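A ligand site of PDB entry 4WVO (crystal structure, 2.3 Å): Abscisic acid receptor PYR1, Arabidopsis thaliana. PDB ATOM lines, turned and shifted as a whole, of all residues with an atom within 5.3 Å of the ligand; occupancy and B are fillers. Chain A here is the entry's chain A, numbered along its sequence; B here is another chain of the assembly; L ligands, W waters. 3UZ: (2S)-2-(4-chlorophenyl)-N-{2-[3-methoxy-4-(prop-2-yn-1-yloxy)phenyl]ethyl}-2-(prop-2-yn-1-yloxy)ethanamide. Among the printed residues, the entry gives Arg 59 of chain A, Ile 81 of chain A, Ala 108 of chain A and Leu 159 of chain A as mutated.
OAN of the ligand sits at hydrogen-bond distance from NE of Arg 59 (2.6 Å).
A nitrogen (NAO) of the ligand is in hydrogen-bond range of the side-chain carboxylate (OE2) of Glu 94.
An oxygen (OAN) of the ligand sits at hydrogen-bond distance from the side-chain amide nitrogen of Asn 167, 3.5 Å away.
The side-chain amide nitrogen (ND2) of Asn 167 sits close to the guanidinium group (NH1) of Arg 59, 3.3 Å away.
The side-chain hydroxyl (OG) of Ser 92 is in hydrogen-bond range of the side-chain carboxylate (OE2) of Glu 94 (2.7 Å).
NH2 of Arg 79 lies within salt-bridge range of OE1 of Glu 94 (2.7 Å).
The backbone NH (N) of Ile 110 lies within hydrogen-bond range of the backbone carbonyl oxygen (O) of Tyr 120, 3.0 Å away.
The backbone carbonyl oxygen of Val 163 lies close to the side-chain amide nitrogen of Asn 167, at 3.5 Å.
A ring nitrogen (ND1) of His 115 sits at hydrogen-bond distance from the backbone NH (N) of Leu 117, 3.1 Å away.
The backbone NH (N) of His 60 is in hydrogen-bond range of the side-chain amide oxygen (OD1) of Asn 167.
O of Ser 92 is in hydrogen-bond range of N of Ile 81 (2.8 Å).
Phe 61 touches the ligand (CB to CAT, 3.6 Å).
Pro 88 touches the ligand.
Ala 89 touches the ligand.
Ser 92 touches the ligand (OG to CAW, 3.8 Å).
CB of Ala 108 touches CAL of the ligand, at 3.2 Å.
Ser 109 touches the ligand (N to CAL, 3.5 Å).
Ile 110 touches the ligand.
His 115 touches the ligand.
CD1 of Leu 117 touches CAB of the ligand, at 3.5 Å.
Tyr 120 touches the ligand.
Ser 122 touches the ligand.
Leu 159 touches the ligand (CD1 to CBC, 3.2 Å).
Val 163 touches the ligand (CG1 to CAF, 3.3 Å).
Gly 218 of chain B touches the ligand (O to CBC, 3.7 Å).
CG2 of Val 219 of chain B touches CBC of the ligand, 3.9 Å away.
Hydrophobic or aromatic side chains that line the ligand: Phe 61, Pro 88, Ala 89, Ala 108, Ile 110, His 115, Leu 117, Tyr 120, Leu 159, Val 163 and Val 219 of chain B.
Of the 27 residues printed, 18 come within 4 Å of the ligand.
The nearest printed residue that does not touch the ligand is Val 83 (4.04 Å).
Water W1 lies within hydrogen-bond range of OAN of the ligand (2.5 Å), ND2 of Asn 167 (2.9 Å) and O of His 60 (2.9 Å).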
ATOM      1  N   ARG A  59      22.182   7.204  35.809  1.00  0.00           N
ATOM      2  CA  ARG A  59      21.472   6.087  35.248  1.00  0.00           C
ATOM      3  C   ARG A  59      22.305   4.857  35.371  1.00  0.00           C
ATOM      4  O   ARG A  59      23.485   4.945  35.434  1.00  0.00           O
ATOM      5  CB  ARG A  59      21.118   6.359  33.789  1.00  0.00           C
ATOM      6  CG  ARG A  59      19.937   7.274  33.641  1.00  0.00           C
ATOM      7  CD  ARG A  59      19.621   7.631  32.232  1.00  0.00           C
ATOM      8  NE  ARG A  59      18.532   6.849  31.725  1.00  0.00           N
ATOM      9  CZ  ARG A  59      17.288   6.961  32.127  1.00  0.00           C
ATOM     10  NH1 ARG A  59      16.372   6.189  31.614  1.00  0.00           N
ATOM     11  NH2 ARG A  59      16.958   7.833  33.027  1.00  0.00           N
ATOM     12  N   HIS A  60      21.655   3.720  35.404  1.00  0.00           N
ATOM     13  CA  HIS A  60      22.316   2.449  35.609  1.00  0.00           C
ATOM     14  C   HIS A  60      22.704   1.782  34.334  1.00  0.00           C
ATOM     15  O   HIS A  60      22.362   2.225  33.283  1.00  0.00           O
ATOM     16  CB  HIS A  60      21.405   1.533  36.381  1.00  0.00           C
ATOM     17  CG  HIS A  60      21.387   1.798  37.842  1.00  0.00           C
ATOM     18  ND1 HIS A  60      20.237   2.087  38.523  1.00  0.00           N
ATOM     19  CD2 HIS A  60      22.380   1.825  38.753  1.00  0.00           C
ATOM     20  CE1 HIS A  60      20.528   2.270  39.790  1.00  0.00           C
ATOM     21  NE2 HIS A  60      21.823   2.111  39.953  1.00  0.00           N
ATOM     22  N   PHE A  61      23.420   0.690  34.471  1.00  0.00           N
ATOM     23  CA  PHE A  61      23.729  -0.208  33.394  1.00  0.00           C
ATOM     24  C   PHE A  61      24.661   0.317  32.315  1.00  0.00           C
ATOM     25  O   PHE A  61      24.806  -0.300  31.312  1.00  0.00           O
ATOM     26  CB  PHE A  61      22.467  -0.759  32.767  1.00  0.00           C
ATOM     27  CG  PHE A  61      21.448  -1.206  33.727  1.00  0.00           C
ATOM     28  CD1 PHE A  61      21.687  -2.256  34.567  1.00  0.00           C
ATOM     29  CD2 PHE A  61      20.222  -0.597  33.767  1.00  0.00           C
ATOM     30  CE1 PHE A  61      20.734  -2.655  35.441  1.00  0.00           C
ATOM     31  CE2 PHE A  61      19.268  -0.999  34.650  1.00  0.00           C
ATOM     32  CZ  PHE A  61      19.531  -2.028  35.487  1.00  0.00           C
ATOM     33  N   ILE A  62      25.296   1.443  32.540  1.00  0.00           N
ATOM     34  CA  ILE A  62      26.192   1.979  31.557  1.00  0.00           C
ATOM     35  C   ILE A  62      27.649   1.736  31.905  1.00  0.00           C
ATOM     36  O   ILE A  62      28.141   2.201  32.904  1.00  0.00           O
ATOM     37  CB  ILE A  62      25.979   3.467  31.364  1.00  0.00           C
ATOM     38  CG1 ILE A  62      24.566   3.752  30.938  1.00  0.00           C
ATOM     39  CG2 ILE A  62      26.919   4.002  30.321  1.00  0.00           C
ATOM     40  CD1 ILE A  62      24.087   5.120  31.309  1.00  0.00           C
ATOM     41  N   ARG A  79      24.542   9.513  21.371  1.00  0.00           N
ATOM     42  CA  ARG A  79      25.504   8.921  22.250  1.00  0.00           C
ATOM     43  C   ARG A  79      25.645   7.450  21.983  1.00  0.00           C
ATOM     44  O   ARG A  79      24.703   6.792  21.670  1.00  0.00           O
ATOM     45  CB  ARG A  79      25.196   9.201  23.706  1.00  0.00           C
ATOM     46  CG  ARG A  79      23.862   8.759  24.197  1.00  0.00           C
ATOM     47  CD  ARG A  79      23.595   9.287  25.584  1.00  0.00           C
ATOM     48  NE  ARG A  79      22.393   8.716  26.127  1.00  0.00           N
ATOM     49  CZ  ARG A  79      21.629   9.273  27.041  1.00  0.00           C
ATOM     50  NH1 ARG A  79      21.933  10.439  27.559  1.00  0.00           N
ATOM     51  NH2 ARG A  79      20.559   8.648  27.441  1.00  0.00           N
ATOM     52  N   ILE A  81      26.620   3.985  23.661  1.00  0.00           N
ATOM     53  CA  ILE A  81      26.771   3.321  24.925  1.00  0.00           C
ATOM     54  C   ILE A  81      27.110   1.855  24.757  1.00  0.00           C
ATOM     55  O   ILE A  81      26.640   1.205  23.891  1.00  0.00           O
ATOM     56  CB  ILE A  81      25.514   3.534  25.775  1.00  0.00           C
ATOM     57  CG1 ILE A  81      25.506   4.930  26.300  1.00  0.00           C
ATOM     58  CG2 ILE A  81      25.420   2.568  26.933  1.00  0.00           C
ATOM     59  CD1 ILE A  81      24.144   5.546  26.396  1.00  0.00           C
ATOM     60  N   VAL A  83      26.700  -1.273  27.366  1.00  0.00           N
ATOM     61  CA  VAL A  83      26.087  -1.617  28.603  1.00  0.00           C
ATOM     62  C   VAL A  83      26.910  -2.641  29.343  1.00  0.00           C
ATOM     63  O   VAL A  83      27.676  -3.333  28.766  1.00  0.00           O
ATOM     64  CB  VAL A  83      24.626  -2.073  28.421  1.00  0.00           C
ATOM     65  CG1 VAL A  83      23.954  -1.267  27.364  1.00  0.00           C
ATOM     66  CG2 VAL A  83      24.516  -3.517  28.073  1.00  0.00           C
ATOM     67  N   LEU A  87      23.170  -8.520  30.588  1.00  0.00           N
ATOM     68  CA  LEU A  87      21.898  -7.918  30.142  1.00  0.00           C
ATOM     69  C   LEU A  87      21.465  -8.394  28.745  1.00  0.00           C
ATOM     70  O   LEU A  87      22.286  -8.869  27.955  1.00  0.00           O
ATOM     71  CB  LEU A  87      22.015  -6.382  30.141  1.00  0.00           C
ATOM     72  CG  LEU A  87      22.209  -5.577  31.433  1.00  0.00           C
ATOM     73  CD1 LEU A  87      22.168  -4.056  31.136  1.00  0.00           C
ATOM     74  CD2 LEU A  87      21.173  -5.924  32.464  1.00  0.00           C
ATOM     75  N   PRO A  88      20.159  -8.244  28.422  1.00  0.00           N
ATOM     76  CA  PRO A  88      19.660  -8.510  27.073  1.00  0.00           C
ATOM     77  C   PRO A  88      19.998  -7.388  26.084  1.00  0.00           C
ATOM     78  O   PRO A  88      19.178  -7.066  25.227  1.00  0.00           O
ATOM     79  CB  PRO A  88      18.143  -8.612  27.288  1.00  0.00           C
ATOM     80  CG  PRO A  88      17.874  -7.721  28.418  1.00  0.00           C
ATOM     81  CD  PRO A  88      19.056  -7.884  29.337  1.00  0.00           C
ATOM     82  N   ALA A  89      21.196  -6.829  26.206  1.00  0.00           N
ATOM     83  CA  ALA A  89      21.666  -5.770  25.321  1.00  0.00           C
ATOM     84  C   ALA A  89      23.182  -5.668  25.421  1.00  0.00           C
ATOM     85  O   ALA A  89      23.750  -5.969  26.477  1.00  0.00           O
ATOM     86  CB  ALA A  89      21.017  -4.447  25.688  1.00  0.00           C
ATOM     87  N   THR A  91      24.919  -2.938  23.251  1.00  0.00           N
ATOM     88  CA  THR A  91      25.162  -1.544  22.913  1.00  0.00           C
ATOM     89  C   THR A  91      23.843  -0.789  22.854  1.00  0.00           C
ATOM     90  O   THR A  91      22.777  -1.385  22.678  1.00  0.00           O
ATOM     91  CB  THR A  91      25.872  -1.406  21.557  1.00  0.00           C
ATOM     92  OG1 THR A  91      25.108  -2.090  20.557  1.00  0.00           O
ATOM     93  CG2 THR A  91      27.259  -2.023  21.598  1.00  0.00           C
ATOM     94  N   SER A  92      23.927   0.529  22.996  1.00  0.00           N
ATOM     95  CA  SER A  92      22.743   1.351  22.789  1.00  0.00           C
ATOM     96  C   SER A  92      23.148   2.662  22.101  1.00  0.00           C
ATOM     97  O   SER A  92      24.105   3.346  22.517  1.00  0.00           O
ATOM     98  CB  SER A  92      22.019   1.598  24.134  1.00  0.00           C
ATOM     99  OG  SER A  92      20.746   2.184  23.955  1.00  0.00           O
ATOM    100  N   GLU A  94      21.739   6.240  21.193  1.00  0.00           N
ATOM    101  CA  GLU A  94      20.650   7.062  21.673  1.00  0.00           C
ATOM    102  C   GLU A  94      20.802   8.491  21.161  1.00  0.00           C
ATOM    103  O   GLU A  94      21.930   8.942  20.964  1.00  0.00           O
ATOM    104  CB  GLU A  94      20.602   6.997  23.199  1.00  0.00           C
ATOM    105  CG  GLU A  94      20.520   5.554  23.679  1.00  0.00           C
ATOM    106  CD  GLU A  94      20.444   5.384  25.172  1.00  0.00           C
ATOM    107  OE1 GLU A  94      20.581   6.403  25.896  1.00  0.00           O
ATOM    108  OE2 GLU A  94      20.245   4.232  25.628  1.00  0.00           O
ATOM    109  N   ALA A 108      15.115  11.687  25.319  1.00  0.00           N
ATOM    110  CA  ALA A 108      15.952  10.930  24.392  1.00  0.00           C
ATOM    111  C   ALA A 108      15.201   9.766  23.782  1.00  0.00           C
ATOM    112  O   ALA A 108      14.159   9.320  24.291  1.00  0.00           O
ATOM    113  CB  ALA A 108      17.245  10.435  25.113  1.00  0.00           C
ATOM    114  N   SER A 109      15.768   9.249  22.701  1.00  0.00           N
ATOM    115  CA  SER A 109      15.246   8.122  21.950  1.00  0.00           C
ATOM    116  C   SER A 109      16.343   7.096  21.744  1.00  0.00           C
ATOM    117  O   SER A 109      17.454   7.441  21.388  1.00  0.00           O
ATOM    118  CB  SER A 109      14.708   8.588  20.590  1.00  0.00           C
ATOM    119  OG  SER A 109      13.544   9.364  20.737  1.00  0.00           O
ATOM    120  N   ILE A 110      16.021   5.828  21.948  1.00  0.00           N
ATOM    121  CA  ILE A 110      16.955   4.768  21.554  1.00  0.00           C
ATOM    122  C   ILE A 110      16.770   4.481  20.052  1.00  0.00           C
ATOM    123  O   ILE A 110      15.730   3.976  19.643  1.00  0.00           O
ATOM    124  CB  ILE A 110      16.726   3.474  22.383  1.00  0.00           C
ATOM    125  CG1 ILE A 110      17.001   3.745  23.875  1.00  0.00           C
ATOM    126  CG2 ILE A 110      17.604   2.346  21.871  1.00  0.00           C
ATOM    127  CD1 ILE A 110      16.593   2.615  24.774  1.00  0.00           C
ATOM    128  N   HIS A 115      19.984  -4.851  20.883  1.00  0.00           N
ATOM    129  CA  HIS A 115      18.960  -5.056  21.905  1.00  0.00           C
ATOM    130  C   HIS A 115      17.592  -5.120  21.240  1.00  0.00           C
ATOM    131  O   HIS A 115      17.473  -4.964  20.013  1.00  0.00           O
ATOM    132  CB  HIS A 115      18.937  -3.893  22.903  1.00  0.00           C
ATOM    133  CG  HIS A 115      18.767  -2.559  22.247  1.00  0.00           C
ATOM    134  ND1 HIS A 115      17.551  -2.135  21.751  1.00  0.00           N
ATOM    135  CD2 HIS A 115      19.672  -1.602  21.926  1.00  0.00           C
ATOM    136  CE1 HIS A 115      17.708  -0.951  21.187  1.00  0.00           C
ATOM    137  NE2 HIS A 115      18.979  -0.601  21.282  1.00  0.00           N
ATOM    138  N   LEU A 117      14.692  -3.348  22.117  1.00  0.00           N
ATOM    139  CA  LEU A 117      13.800  -2.188  22.241  1.00  0.00           C
ATOM    140  C   LEU A 117      13.657  -1.485  20.895  1.00  0.00           C
ATOM    141  O   LEU A 117      14.656  -1.064  20.292  1.00  0.00           O
ATOM    142  CB  LEU A 117      14.302  -1.201  23.283  1.00  0.00           C
ATOM    143  CG  LEU A 117      14.432  -1.724  24.704  1.00  0.00           C
ATOM    144  CD1 LEU A 117      14.981  -0.633  25.582  1.00  0.00           C
ATOM    145  CD2 LEU A 117      13.095  -2.231  25.237  1.00  0.00           C
ATOM    146  N   TYR A 120      11.777   3.103  21.516  1.00  0.00           N
ATOM    147  CA  TYR A 120      11.800   3.651  22.865  1.00  0.00           C
ATOM    148  C   TYR A 120      12.087   5.166  22.817  1.00  0.00           C
ATOM    149  O   TYR A 120      12.997   5.602  22.130  1.00  0.00           O
ATOM    150  CB  TYR A 120      12.847   2.954  23.760  1.00  0.00           C
ATOM    151  CG  TYR A 120      12.738   3.339  25.229  1.00  0.00           C
ATOM    152  CD1 TYR A 120      13.344   4.510  25.706  1.00  0.00           C
ATOM    153  CD2 TYR A 120      12.027   2.556  26.118  1.00  0.00           C
ATOM    154  CE1 TYR A 120      13.237   4.880  27.035  1.00  0.00           C
ATOM    155  CE2 TYR A 120      11.919   2.922  27.457  1.00  0.00           C
ATOM    156  CZ  TYR A 120      12.516   4.080  27.908  1.00  0.00           C
ATOM    157  OH  TYR A 120      12.407   4.436  29.233  1.00  0.00           O
ATOM    158  N   SER A 122      12.005   8.582  25.684  1.00  0.00           N
ATOM    159  CA  SER A 122      11.659   9.030  27.021  1.00  0.00           C
ATOM    160  C   SER A 122      11.665  10.558  27.116  1.00  0.00           C
ATOM    161  O   SER A 122      12.261  11.235  26.281  1.00  0.00           O
ATOM    162  CB  SER A 122      12.594   8.428  28.063  1.00  0.00           C
ATOM    163  OG  SER A 122      13.918   8.927  27.945  1.00  0.00           O
ATOM    164  N   LEU A 159       9.581  -4.393  32.203  1.00  0.00           N
ATOM    165  CA  LEU A 159      10.972  -4.170  31.985  1.00  0.00           C
ATOM    166  C   LEU A 159      11.305  -2.703  32.073  1.00  0.00           C
ATOM    167  O   LEU A 159      12.179  -2.318  32.791  1.00  0.00           O
ATOM    168  CB  LEU A 159      11.351  -4.694  30.638  1.00  0.00           C
ATOM    169  CG  LEU A 159      12.748  -4.426  30.152  1.00  0.00           C
ATOM    170  CD1 LEU A 159      13.795  -4.612  31.201  1.00  0.00           C
ATOM    171  CD2 LEU A 159      13.041  -5.309  28.963  1.00  0.00           C
ATOM    172  N   ALA A 160      10.582  -1.900  31.335  1.00  0.00           N
ATOM    173  CA  ALA A 160      10.806  -0.478  31.298  1.00  0.00           C
ATOM    174  C   ALA A 160      10.536   0.225  32.601  1.00  0.00           C
ATOM    175  O   ALA A 160      11.281   1.074  32.980  1.00  0.00           O
ATOM    176  CB  ALA A 160       9.995   0.136  30.194  1.00  0.00           C
ATOM    177  N   VAL A 163      13.461  -0.445  34.968  1.00  0.00           N
ATOM    178  CA  VAL A 163      14.630   0.348  34.635  1.00  0.00           C
ATOM    179  C   VAL A 163      14.411   1.798  35.048  1.00  0.00           C
ATOM    180  O   VAL A 163      15.240   2.376  35.737  1.00  0.00           O
ATOM    181  CB  VAL A 163      14.957   0.252  33.131  1.00  0.00           C
ATOM    182  CG1 VAL A 163      16.041   1.252  32.741  1.00  0.00           C
ATOM    183  CG2 VAL A 163      15.361  -1.198  32.742  1.00  0.00           C
ATOM    184  N   VAL A 164      13.272   2.387  34.658  1.00  0.00           N
ATOM    185  CA  VAL A 164      13.062   3.812  34.886  1.00  0.00           C
ATOM    186  C   VAL A 164      12.971   4.126  36.387  1.00  0.00           C
ATOM    187  O   VAL A 164      13.551   5.097  36.844  1.00  0.00           O
ATOM    188  CB  VAL A 164      11.794   4.333  34.143  1.00  0.00           C
ATOM    189  CG1 VAL A 164      11.431   5.776  34.586  1.00  0.00           C
ATOM    190  CG2 VAL A 164      11.984   4.282  32.643  1.00  0.00           C
ATOM    191  N   ASN A 167      16.440   4.060  37.884  1.00  0.00           N
ATOM    192  CA  ASN A 167      17.232   5.212  37.457  1.00  0.00           C
ATOM    193  C   ASN A 167      16.777   6.458  38.189  1.00  0.00           C
ATOM    194  O   ASN A 167      17.585   7.339  38.488  1.00  0.00           O
ATOM    195  CB  ASN A 167      17.161   5.400  35.939  1.00  0.00           C
ATOM    196  CG  ASN A 167      17.987   4.381  35.194  1.00  0.00           C
ATOM    197  OD1 ASN A 167      18.931   3.804  35.742  1.00  0.00           O
ATOM    198  ND2 ASN A 167      17.649   4.158  33.932  1.00  0.00           N
ATOM    199  N   GLY B 218      12.923  -8.986  33.204  1.00  0.00           N
ATOM    200  CA  GLY B 218      13.588  -8.790  31.947  1.00  0.00           C
ATOM    201  C   GLY B 218      15.020  -8.351  32.048  1.00  0.00           C
ATOM    202  O   GLY B 218      15.568  -7.959  31.093  1.00  0.00           O
ATOM    203  N   VAL B 219      15.608  -8.417  33.229  1.00  0.00           N
ATOM    204  CA  VAL B 219      16.966  -7.991  33.405  1.00  0.00           C
ATOM    205  C   VAL B 219      17.945  -9.125  33.619  1.00  0.00           C
ATOM    206  O   VAL B 219      18.716  -9.401  32.760  1.00  0.00           O
ATOM    207  CB  VAL B 219      17.102  -6.952  34.522  1.00  0.00           C
ATOM    208  CG1 VAL B 219      18.543  -6.545  34.678  1.00  0.00           C
ATOM    209  CG2 VAL B 219      16.257  -5.731  34.239  1.00  0.00           C
HETATM  210  CAC 3UZ L   1      17.163   2.037  28.436  1.00  0.00           C
HETATM  211  CAB 3UZ L   1      16.509   0.811  28.442  1.00  0.00           C
HETATM  212  CAA 3UZ L   1      15.283   0.679  29.095  1.00  0.00           C
HETATM  213 CL1  3UZ L   1      14.482  -0.850  29.105  1.00  0.00          CL
HETATM  214  CAF 3UZ L   1      14.718   1.767  29.731  1.00  0.00           C
HETATM  215  CAE 3UZ L   1      15.366   3.000  29.727  1.00  0.00           C
HETATM  216  CAD 3UZ L   1      16.592   3.132  29.074  1.00  0.00           C
HETATM  217  CAH 3UZ L   1      17.246   4.358  29.068  1.00  0.00           C
HETATM  218  OAI 3UZ L   1      17.257   4.882  27.730  1.00  0.00           O
HETATM  219  CAJ 3UZ L   1      17.259   6.311  27.785  1.00  0.00           C
HETATM  220  CAK 3UZ L   1      16.892   6.840  26.465  1.00  0.00           C
HETATM  221  CAL 3UZ L   1      16.598   7.269  25.414  1.00  0.00           C
HETATM  222  CAM 3UZ L   1      18.678   4.175  29.568  1.00  0.00           C
HETATM  223  OAN 3UZ L   1      18.984   4.448  30.727  1.00  0.00           O
HETATM  224  NAO 3UZ L   1      19.548   3.717  28.650  1.00  0.00           N
HETATM  225  CAP 3UZ L   1      20.965   3.488  28.967  1.00  0.00           C
HETATM  226  CAQ 3UZ L   1      21.527   2.422  28.023  1.00  0.00           C
HETATM  227  CAR 3UZ L   1      20.896   1.204  28.284  1.00  0.00           C
HETATM  228  CAW 3UZ L   1      20.129   0.605  27.300  1.00  0.00           C
HETATM  229  CAV 3UZ L   1      19.505  -0.610  27.572  1.00  0.00           C
HETATM  230  OAX 3UZ L   1      18.730  -1.258  26.656  1.00  0.00           O
HETATM  231  CAY 3UZ L   1      19.519  -1.563  25.496  1.00  0.00           C
HETATM  232  CAS 3UZ L   1      21.054   0.592  29.523  1.00  0.00           C
HETATM  233  CAT 3UZ L   1      20.430  -0.623  29.796  1.00  0.00           C
HETATM  234  CAU 3UZ L   1      19.657  -1.211  28.803  1.00  0.00           C
HETATM  235  OAZ 3UZ L   1      19.017  -2.404  28.988  1.00  0.00           O
HETATM  236  CBA 3UZ L   1      18.145  -2.301  30.112  1.00  0.00           C
HETATM  237  CBB 3UZ L   1      17.483  -3.601  30.336  1.00  0.00           C
HETATM  238  CBC 3UZ L   1      16.950  -4.626  30.515  1.00  0.00           C
HETATM  239  O   HOH W   1      19.617   2.714  32.392  1.00  0.00           O
HETATM  240  O   HOH W   2      17.515  -3.608  26.882  1.00  0.00           O
